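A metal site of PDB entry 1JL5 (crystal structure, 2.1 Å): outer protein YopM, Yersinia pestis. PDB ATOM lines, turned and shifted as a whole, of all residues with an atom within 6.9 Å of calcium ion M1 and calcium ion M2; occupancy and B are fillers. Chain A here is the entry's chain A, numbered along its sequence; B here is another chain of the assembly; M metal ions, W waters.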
ATOM      1  N   ASN A 224     -13.022   9.134  21.294  1.00  0.00           N
ATOM      2  CA  ASN A 224     -12.215   7.999  20.933  1.00  0.00           C
ATOM      3  C   ASN A 224     -10.900   7.891  21.642  1.00  0.00           C
ATOM      4  O   ASN A 224      -9.859   7.642  21.042  1.00  0.00           O
ATOM      5  CB  ASN A 224     -11.979   7.972  19.444  1.00  0.00           C
ATOM      6  CG  ASN A 224     -13.001   7.142  18.748  1.00  0.00           C
ATOM      7  OD1 ASN A 224     -13.126   5.953  19.033  1.00  0.00           O
ATOM      8  ND2 ASN A 224     -13.757   7.751  17.847  1.00  0.00           N
ATOM      9  N   ASP A 245     -16.919  11.738  22.932  1.00  0.00           N
ATOM     10  CA  ASP A 245     -17.582  10.577  22.399  1.00  0.00           C
ATOM     11  C   ASP A 245     -16.598   9.434  22.422  1.00  0.00           C
ATOM     12  O   ASP A 245     -15.394   9.643  22.544  1.00  0.00           O
ATOM     13  CB  ASP A 245     -17.993  10.825  20.956  1.00  0.00           C
ATOM     14  CG  ASP A 245     -16.812  11.220  20.090  1.00  0.00           C
ATOM     15  OD1 ASP A 245     -16.315  12.361  20.250  1.00  0.00           O
ATOM     16  OD2 ASP A 245     -16.355  10.401  19.277  1.00  0.00           O
ATOM     17  N   ASN A 246     -17.114   8.220  22.328  1.00  0.00           N
ATOM     18  CA  ASN A 246     -16.266   7.054  22.260  1.00  0.00           C
ATOM     19  C   ASN A 246     -15.190   6.985  23.305  1.00  0.00           C
ATOM     20  O   ASN A 246     -14.020   6.785  22.997  1.00  0.00           O
ATOM     21  CB  ASN A 246     -15.659   6.972  20.874  1.00  0.00           C
ATOM     22  CG  ASN A 246     -16.697   6.679  19.838  1.00  0.00           C
ATOM     23  OD1 ASN A 246     -17.258   5.586  19.826  1.00  0.00           O
ATOM     24  ND2 ASN A 246     -16.987   7.651  18.984  1.00  0.00           N
ATOM     25  N   ASN A 247     -15.604   7.158  24.547  1.00  0.00           N
ATOM     26  CA  ASN A 247     -14.673   7.061  25.641  1.00  0.00           C
ATOM     27  C   ASN A 247     -15.250   6.069  26.605  1.00  0.00           C
ATOM     28  O   ASN A 247     -16.055   5.227  26.215  1.00  0.00           O
ATOM     29  CB  ASN A 247     -14.463   8.436  26.272  1.00  0.00           C
ATOM     30  CG  ASN A 247     -13.438   9.241  25.522  1.00  0.00           C
ATOM     31  OD1 ASN A 247     -12.272   8.864  25.458  1.00  0.00           O
ATOM     32  ND2 ASN A 247     -13.856  10.362  24.946  1.00  0.00           N
ATOM     33  N   ARG A 265     -21.157  10.910  22.475  1.00  0.00           N
ATOM     34  CA  ARG A 265     -21.668   9.759  21.762  1.00  0.00           C
ATOM     35  C   ARG A 265     -20.843   8.558  22.153  1.00  0.00           C
ATOM     36  O   ARG A 265     -19.629   8.630  22.300  1.00  0.00           O
ATOM     37  CB  ARG A 265     -21.568   9.990  20.254  1.00  0.00           C
ATOM     38  CG  ARG A 265     -21.790   8.743  19.416  1.00  0.00           C
ATOM     39  CD  ARG A 265     -21.695   9.111  17.953  1.00  0.00           C
ATOM     40  NE  ARG A 265     -21.636   7.957  17.058  1.00  0.00           N
ATOM     41  CZ  ARG A 265     -22.670   7.183  16.745  1.00  0.00           C
ATOM     42  NH1 ARG A 265     -23.875   7.430  17.253  1.00  0.00           N
ATOM     43  NH2 ARG A 265     -22.497   6.161  15.914  1.00  0.00           N
ATOM     44  N   ASP A 266     -21.534   7.453  22.322  1.00  0.00           N
ATOM     45  CA  ASP A 266     -20.904   6.205  22.667  1.00  0.00           C
ATOM     46  C   ASP A 266     -20.059   6.287  23.913  1.00  0.00           C
ATOM     47  O   ASP A 266     -18.826   6.326  23.880  1.00  0.00           O
ATOM     48  CB  ASP A 266     -20.064   5.686  21.521  1.00  0.00           C
ATOM     49  CG  ASP A 266     -19.705   4.231  21.709  1.00  0.00           C
ATOM     50  OD1 ASP A 266     -20.007   3.707  22.801  1.00  0.00           O
ATOM     51  OD2 ASP A 266     -19.151   3.625  20.780  1.00  0.00           O
ATOM     52  N   ASN A 267     -20.751   6.316  25.040  1.00  0.00           N
ATOM     53  CA  ASN A 267     -20.117   6.322  26.328  1.00  0.00           C
ATOM     54  C   ASN A 267     -21.071   5.513  27.153  1.00  0.00           C
ATOM     55  O   ASN A 267     -21.945   4.849  26.604  1.00  0.00           O
ATOM     56  CB  ASN A 267     -19.947   7.736  26.857  1.00  0.00           C
ATOM     57  CG  ASN A 267     -18.676   8.368  26.339  1.00  0.00           C
ATOM     58  OD1 ASN A 267     -17.573   7.950  26.699  1.00  0.00           O
ATOM     59  ND2 ASN A 267     -18.806   9.373  25.477  1.00  0.00           N
ATOM     60  N   TYR A 268     -20.939   5.552  28.457  1.00  0.00           N
ATOM     61  CA  TYR A 268     -21.802   4.737  29.268  1.00  0.00           C
ATOM     62  C   TYR A 268     -22.679   5.623  30.105  1.00  0.00           C
ATOM     63  O   TYR A 268     -22.904   5.344  31.282  1.00  0.00           O
ATOM     64  CB  TYR A 268     -20.960   3.839  30.154  1.00  0.00           C
ATOM     65  CG  TYR A 268     -21.637   2.554  30.507  1.00  0.00           C
ATOM     66  CD1 TYR A 268     -21.929   1.615  29.527  1.00  0.00           C
ATOM     67  CD2 TYR A 268     -21.967   2.264  31.827  1.00  0.00           C
ATOM     68  CE1 TYR A 268     -22.526   0.406  29.849  1.00  0.00           C
ATOM     69  CE2 TYR A 268     -22.569   1.064  32.159  1.00  0.00           C
ATOM     70  CZ  TYR A 268     -22.845   0.142  31.170  1.00  0.00           C
ATOM     71  OH  TYR A 268     -23.432  -1.041  31.504  1.00  0.00           O
ATOM     72  N   GLU A 286     -25.706   6.462  21.482  1.00  0.00           N
ATOM     73  CA  GLU A 286     -24.915   5.332  21.923  1.00  0.00           C
ATOM     74  C   GLU A 286     -24.442   5.412  23.354  1.00  0.00           C
ATOM     75  O   GLU A 286     -23.289   5.177  23.655  1.00  0.00           O
ATOM     76  CB  GLU A 286     -23.707   5.134  21.026  1.00  0.00           C
ATOM     77  CG  GLU A 286     -24.047   4.459  19.722  1.00  0.00           C
ATOM     78  CD  GLU A 286     -22.814   4.150  18.932  1.00  0.00           C
ATOM     79  OE1 GLU A 286     -21.942   3.420  19.435  1.00  0.00           O
ATOM     80  OE2 GLU A 286     -22.701   4.641  17.806  1.00  0.00           O
ATOM     81  N   ASN A 287     -25.355   5.796  24.228  1.00  0.00           N
ATOM     82  CA  ASN A 287     -25.029   5.795  25.615  1.00  0.00           C
ATOM     83  C   ASN A 287     -26.061   4.860  26.169  1.00  0.00           C
ATOM     84  O   ASN A 287     -26.580   4.030  25.428  1.00  0.00           O
ATOM     85  CB  ASN A 287     -25.119   7.199  26.187  1.00  0.00           C
ATOM     86  CG  ASN A 287     -23.810   7.929  26.025  1.00  0.00           C
ATOM     87  OD1 ASN A 287     -22.902   7.740  26.813  1.00  0.00           O
ATOM     88  ND2 ASN A 287     -23.705   8.740  24.981  1.00  0.00           N
ATOM     89  N   ILE A 288     -26.375   4.965  27.445  1.00  0.00           N
ATOM     90  CA  ILE A 288     -27.341   4.036  27.963  1.00  0.00           C
ATOM     91  C   ILE A 288     -28.483   4.761  28.625  1.00  0.00           C
ATOM     92  O   ILE A 288     -28.956   4.394  29.692  1.00  0.00           O
ATOM     93  CB  ILE A 288     -26.672   3.045  28.913  1.00  0.00           C
ATOM     94  CG1 ILE A 288     -26.029   3.769  30.100  1.00  0.00           C
ATOM     95  CG2 ILE A 288     -25.579   2.301  28.157  1.00  0.00           C
ATOM     96  CD1 ILE A 288     -25.434   2.812  31.127  1.00  0.00           C
ATOM     97  N   ASN B 287     -26.194  -3.625  23.796  1.00  0.00           N
ATOM     98  CA  ASN B 287     -26.708  -3.731  25.121  1.00  0.00           C
ATOM     99  C   ASN B 287     -25.768  -2.849  25.883  1.00  0.00           C
ATOM    100  O   ASN B 287     -25.156  -1.966  25.288  1.00  0.00           O
ATOM    101  CB  ASN B 287     -26.690  -5.177  25.586  1.00  0.00           C
ATOM    102  CG  ASN B 287     -27.960  -5.885  25.189  1.00  0.00           C
ATOM    103  OD1 ASN B 287     -28.973  -5.744  25.857  1.00  0.00           O
ATOM    104  ND2 ASN B 287     -27.917  -6.610  24.080  1.00  0.00           N
ATOM    105  N   PHE B 289     -23.159  -3.946  27.957  1.00  0.00           N
ATOM    106  CA  PHE B 289     -22.124  -4.772  28.527  1.00  0.00           C
ATOM    107  C   PHE B 289     -20.843  -3.958  28.548  1.00  0.00           C
ATOM    108  O   PHE B 289     -20.477  -3.344  27.544  1.00  0.00           O
ATOM    109  CB  PHE B 289     -21.913  -6.016  27.670  1.00  0.00           C
ATOM    110  CG  PHE B 289     -23.031  -6.992  27.784  1.00  0.00           C
ATOM    111  CD1 PHE B 289     -23.081  -7.867  28.860  1.00  0.00           C
ATOM    112  CD2 PHE B 289     -24.041  -7.026  26.840  1.00  0.00           C
ATOM    113  CE1 PHE B 289     -24.139  -8.754  29.002  1.00  0.00           C
ATOM    114  CE2 PHE B 289     -25.103  -7.904  26.973  1.00  0.00           C
ATOM    115  CZ  PHE B 289     -25.153  -8.779  28.058  1.00  0.00           C
ATOM    116  N   SER B 306     -21.320  -2.798  19.603  1.00  0.00           N
ATOM    117  CA  SER B 306     -22.064  -1.671  20.148  1.00  0.00           C
ATOM    118  C   SER B 306     -22.522  -1.831  21.584  1.00  0.00           C
ATOM    119  O   SER B 306     -23.666  -1.568  21.927  1.00  0.00           O
ATOM    120  CB  SER B 306     -23.242  -1.353  19.246  1.00  0.00           C
ATOM    121  OG  SER B 306     -22.731  -0.861  18.017  1.00  0.00           O
ATOM    122  N   ASN B 307     -21.607  -2.310  22.411  1.00  0.00           N
ATOM    123  CA  ASN B 307     -21.859  -2.440  23.823  1.00  0.00           C
ATOM    124  C   ASN B 307     -20.833  -1.476  24.334  1.00  0.00           C
ATOM    125  O   ASN B 307     -20.471  -0.542  23.633  1.00  0.00           O
ATOM    126  CB  ASN B 307     -21.588  -3.868  24.287  1.00  0.00           C
ATOM    127  CG  ASN B 307     -22.809  -4.733  24.188  1.00  0.00           C
ATOM    128  OD1 ASN B 307     -23.739  -4.581  24.972  1.00  0.00           O
ATOM    129  ND2 ASN B 307     -22.836  -5.629  23.197  1.00  0.00           N
ATOM    130  N   GLU B 308     -20.354  -1.683  25.542  1.00  0.00           N
ATOM    131  CA  GLU B 308     -19.335  -0.809  26.059  1.00  0.00           C
ATOM    132  C   GLU B 308     -18.249  -1.764  26.518  1.00  0.00           C
ATOM    133  O   GLU B 308     -17.608  -1.557  27.533  1.00  0.00           O
ATOM    134  CB  GLU B 308     -19.882   0.024  27.218  1.00  0.00           C
ATOM    135  CG  GLU B 308     -18.989   1.195  27.547  1.00  0.00           C
ATOM    136  CD  GLU B 308     -19.006   2.259  26.474  1.00  0.00           C
ATOM    137  OE1 GLU B 308     -19.399   1.950  25.321  1.00  0.00           O
ATOM    138  OE2 GLU B 308     -18.627   3.393  26.776  1.00  0.00           O
ATOM    139  N   ILE B 309     -18.084  -2.833  25.744  1.00  0.00           N
ATOM    140  CA  ILE B 309     -17.111  -3.854  26.072  1.00  0.00           C
ATOM    141  C   ILE B 309     -15.708  -3.293  26.122  1.00  0.00           C
ATOM    142  O   ILE B 309     -15.166  -2.844  25.114  1.00  0.00           O
ATOM    143  CB  ILE B 309     -17.109  -4.997  25.034  1.00  0.00           C
ATOM    144  CG1 ILE B 309     -18.523  -5.595  24.912  1.00  0.00           C
ATOM    145  CG2 ILE B 309     -16.099  -6.048  25.443  1.00  0.00           C
ATOM    146  CD1 ILE B 309     -19.074  -6.083  26.199  1.00  0.00           C
ATOM    147  N   ASN B 326     -17.544  -1.718  17.419  1.00  0.00           N
ATOM    148  CA  ASN B 326     -18.060  -0.609  18.170  1.00  0.00           C
ATOM    149  C   ASN B 326     -18.175  -0.878  19.656  1.00  0.00           C
ATOM    150  O   ASN B 326     -19.256  -0.872  20.233  1.00  0.00           O
ATOM    151  CB  ASN B 326     -19.426  -0.198  17.620  1.00  0.00           C
ATOM    152  CG  ASN B 326     -19.914   1.086  18.229  1.00  0.00           C
ATOM    153  OD1 ASN B 326     -19.104   1.952  18.570  1.00  0.00           O
ATOM    154  ND2 ASN B 326     -21.220   1.232  18.365  1.00  0.00           N
ATOM    155  N   ASN B 327     -17.034  -1.121  20.267  1.00  0.00           N
ATOM    156  CA  ASN B 327     -16.997  -1.327  21.696  1.00  0.00           C
ATOM    157  C   ASN B 327     -15.869  -0.473  22.179  1.00  0.00           C
ATOM    158  O   ASN B 327     -15.495   0.476  21.511  1.00  0.00           O
ATOM    159  CB  ASN B 327     -16.792  -2.803  22.023  1.00  0.00           C
ATOM    160  CG  ASN B 327     -18.113  -3.537  22.093  1.00  0.00           C
ATOM    161  OD1 ASN B 327     -18.930  -3.254  22.960  1.00  0.00           O
ATOM    162  ND2 ASN B 327     -18.327  -4.467  21.168  1.00  0.00           N
ATOM    163  N   LYS B 328     -15.323  -0.782  23.339  1.00  0.00           N
ATOM    164  CA  LYS B 328     -14.247   0.029  23.867  1.00  0.00           C
ATOM    165  C   LYS B 328     -13.058  -0.850  24.155  1.00  0.00           C
ATOM    166  O   LYS B 328     -12.334  -0.652  25.126  1.00  0.00           O
ATOM    167  CB  LYS B 328     -14.724   0.749  25.126  1.00  0.00           C
ATOM    168  CG  LYS B 328     -15.921   1.646  24.848  1.00  0.00           C
ATOM    169  CD  LYS B 328     -15.545   2.761  23.885  1.00  0.00           C
ATOM    170  CE  LYS B 328     -16.775   3.496  23.378  1.00  0.00           C
ATOM    171  NZ  LYS B 328     -17.618   4.058  24.475  1.00  0.00           N
ATOM    172  N   PHE B 346     -14.292  -0.222  14.945  1.00  0.00           N
ATOM    173  CA  PHE B 346     -14.798   0.770  15.883  1.00  0.00           C
ATOM    174  C   PHE B 346     -14.518   0.393  17.322  1.00  0.00           C
ATOM    175  O   PHE B 346     -15.415   0.320  18.159  1.00  0.00           O
ATOM    176  CB  PHE B 346     -16.296   0.961  15.656  1.00  0.00           C
ATOM    177  CG  PHE B 346     -16.624   1.490  14.310  1.00  0.00           C
ATOM    178  CD1 PHE B 346     -16.324   2.815  13.992  1.00  0.00           C
ATOM    179  CD2 PHE B 346     -17.222   0.685  13.354  1.00  0.00           C
ATOM    180  CE1 PHE B 346     -16.619   3.325  12.738  1.00  0.00           C
ATOM    181  CE2 PHE B 346     -17.526   1.191  12.099  1.00  0.00           C
ATOM    182  CZ  PHE B 346     -17.222   2.506  11.781  1.00  0.00           C
ATOM    183  N   ASN B 347     -13.259   0.147  17.580  1.00  0.00           N
ATOM    184  CA  ASN B 347     -12.820  -0.175  18.922  1.00  0.00           C
ATOM    185  C   ASN B 347     -11.553   0.610  19.111  1.00  0.00           C
ATOM    186  O   ASN B 347     -11.209   1.430  18.274  1.00  0.00           O
ATOM    187  CB  ASN B 347     -12.568  -1.672  19.050  1.00  0.00           C
ATOM    188  CG  ASN B 347     -13.812  -2.421  19.426  1.00  0.00           C
ATOM    189  OD1 ASN B 347     -14.291  -2.306  20.551  1.00  0.00           O
ATOM    190  ND2 ASN B 347     -14.364  -3.155  18.486  1.00  0.00           N
HETATM  191 CA    CA M   1     -18.038   3.851  19.101  1.00  0.00          CA
HETATM  192 CA    CA M   2     -20.748   1.712  23.483  1.00  0.00          CA
HETATM  193  O   HOH W   1     -22.096   1.928  21.632  1.00  0.00           O
HETATM  194  O   HOH W   2     -22.215   3.062  24.970  1.00  0.00           O
HETATM  195  O   HOH W   3     -17.027   4.199  17.148  1.00  0.00           O
HETATM  196  O   HOH W   4     -19.011   1.282  21.941  1.00  0.00           O
HETATM  197  O   HOH W   5     -23.157   0.493  24.271  1.00  0.00           O
HETATM  198  O   HOH W   6     -19.883   4.706  18.244  1.00  0.00           O
HETATM  199  O   HOH W   7     -16.458   2.411  20.016  1.00  0.00           O
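OD2 of Asp 266 binds calcium ion M1. OD1 of Asn 246 is bound to calcium ion M1 (2.0 Å). Water W6 is bound to calcium ion M1 (2.2 Å). Water W3 is bound to calcium ion M1 (2.2 Å). OD1 of Asn 326 of chain B binds calcium ion M1 (2.2 Å). Water W7 is bound to calcium ion M1. Calcium ion M1 has six donor atoms within binding distance.
Water W7 bridges the backbone carbonyl oxygen (O) of Asn 327 of chain B (2.6 Å) and the backbone carbonyl oxygen (O) of Phe 346 of chain B (3.0 Å). Water W5 bridges O of Ser 306 of chain B and O of Asn 287 of chain B. Water W1 lies within hydrogen-bond range of the side-chain carboxylate (OE1) of Glu 286 (2.7 Å) and the side-chain amide nitrogen (ND2) of Asn 326 of chain B (3.5 Å). Water W2 lies within hydrogen-bond range of O of Asn 267 (2.4 Å) and O of Glu 286 (2.7 Å).
OD1 of Asn 307 of chain B lies close to N of Asn 287 of chain B, 2.9 Å away. N of Asn 246 is in hydrogen-bond range of O of Arg 265, 2.5 Å away. The backbone NH of Glu 308 of chain B lies within hydrogen-bond range of the side-chain amide oxygen of Asn 327 of chain B, at 3.3 Å. NH2 of Arg 265 lies within salt-bridge range of OE2 of Glu 286, 2.4 Å away. O of Phe 289 of chain B lies within hydrogen-bond range of N of Glu 308 of chain B. The side-chain hydroxyl of Ser 306 of chain B is in hydrogen-bond range of the side-chain amide nitrogen of Asn 326 of chain B (2.6 Å). N of Asn 247 lies within hydrogen-bond range of O of Asp 266 (3.4 Å). The backbone NH (N) of Phe 289 of chain B lies close to the side-chain amide oxygen (OD1) of Asn 307 of chain B (3.1 Å).
Merely in contact with calcium ion M1: Glu 286. Of the 22 residues printed, 4 come within 4 Å of calcium ion M1.
Calcium ion M2 is bound by OD1 of Asp 266, at 2.2 Å. Calcium ion M2 is bound by O of Asn 307 of chain B (2.3 Å). Calcium ion M2 is bound by OE1 of Glu 308 of chain B, 2.3 Å away. Water W1 is bound to calcium ion M2. Water W4 is bound to calcium ion M2. Water W2 is bound to calcium ion M2 (2.5 Å). Water W5 binds calcium ion M2 (2.8 Å). Calcium ion M2 has seven donor atoms within binding distance.
Of the 22 residues printed, 3 come within 4 Å of calcium ion M2.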
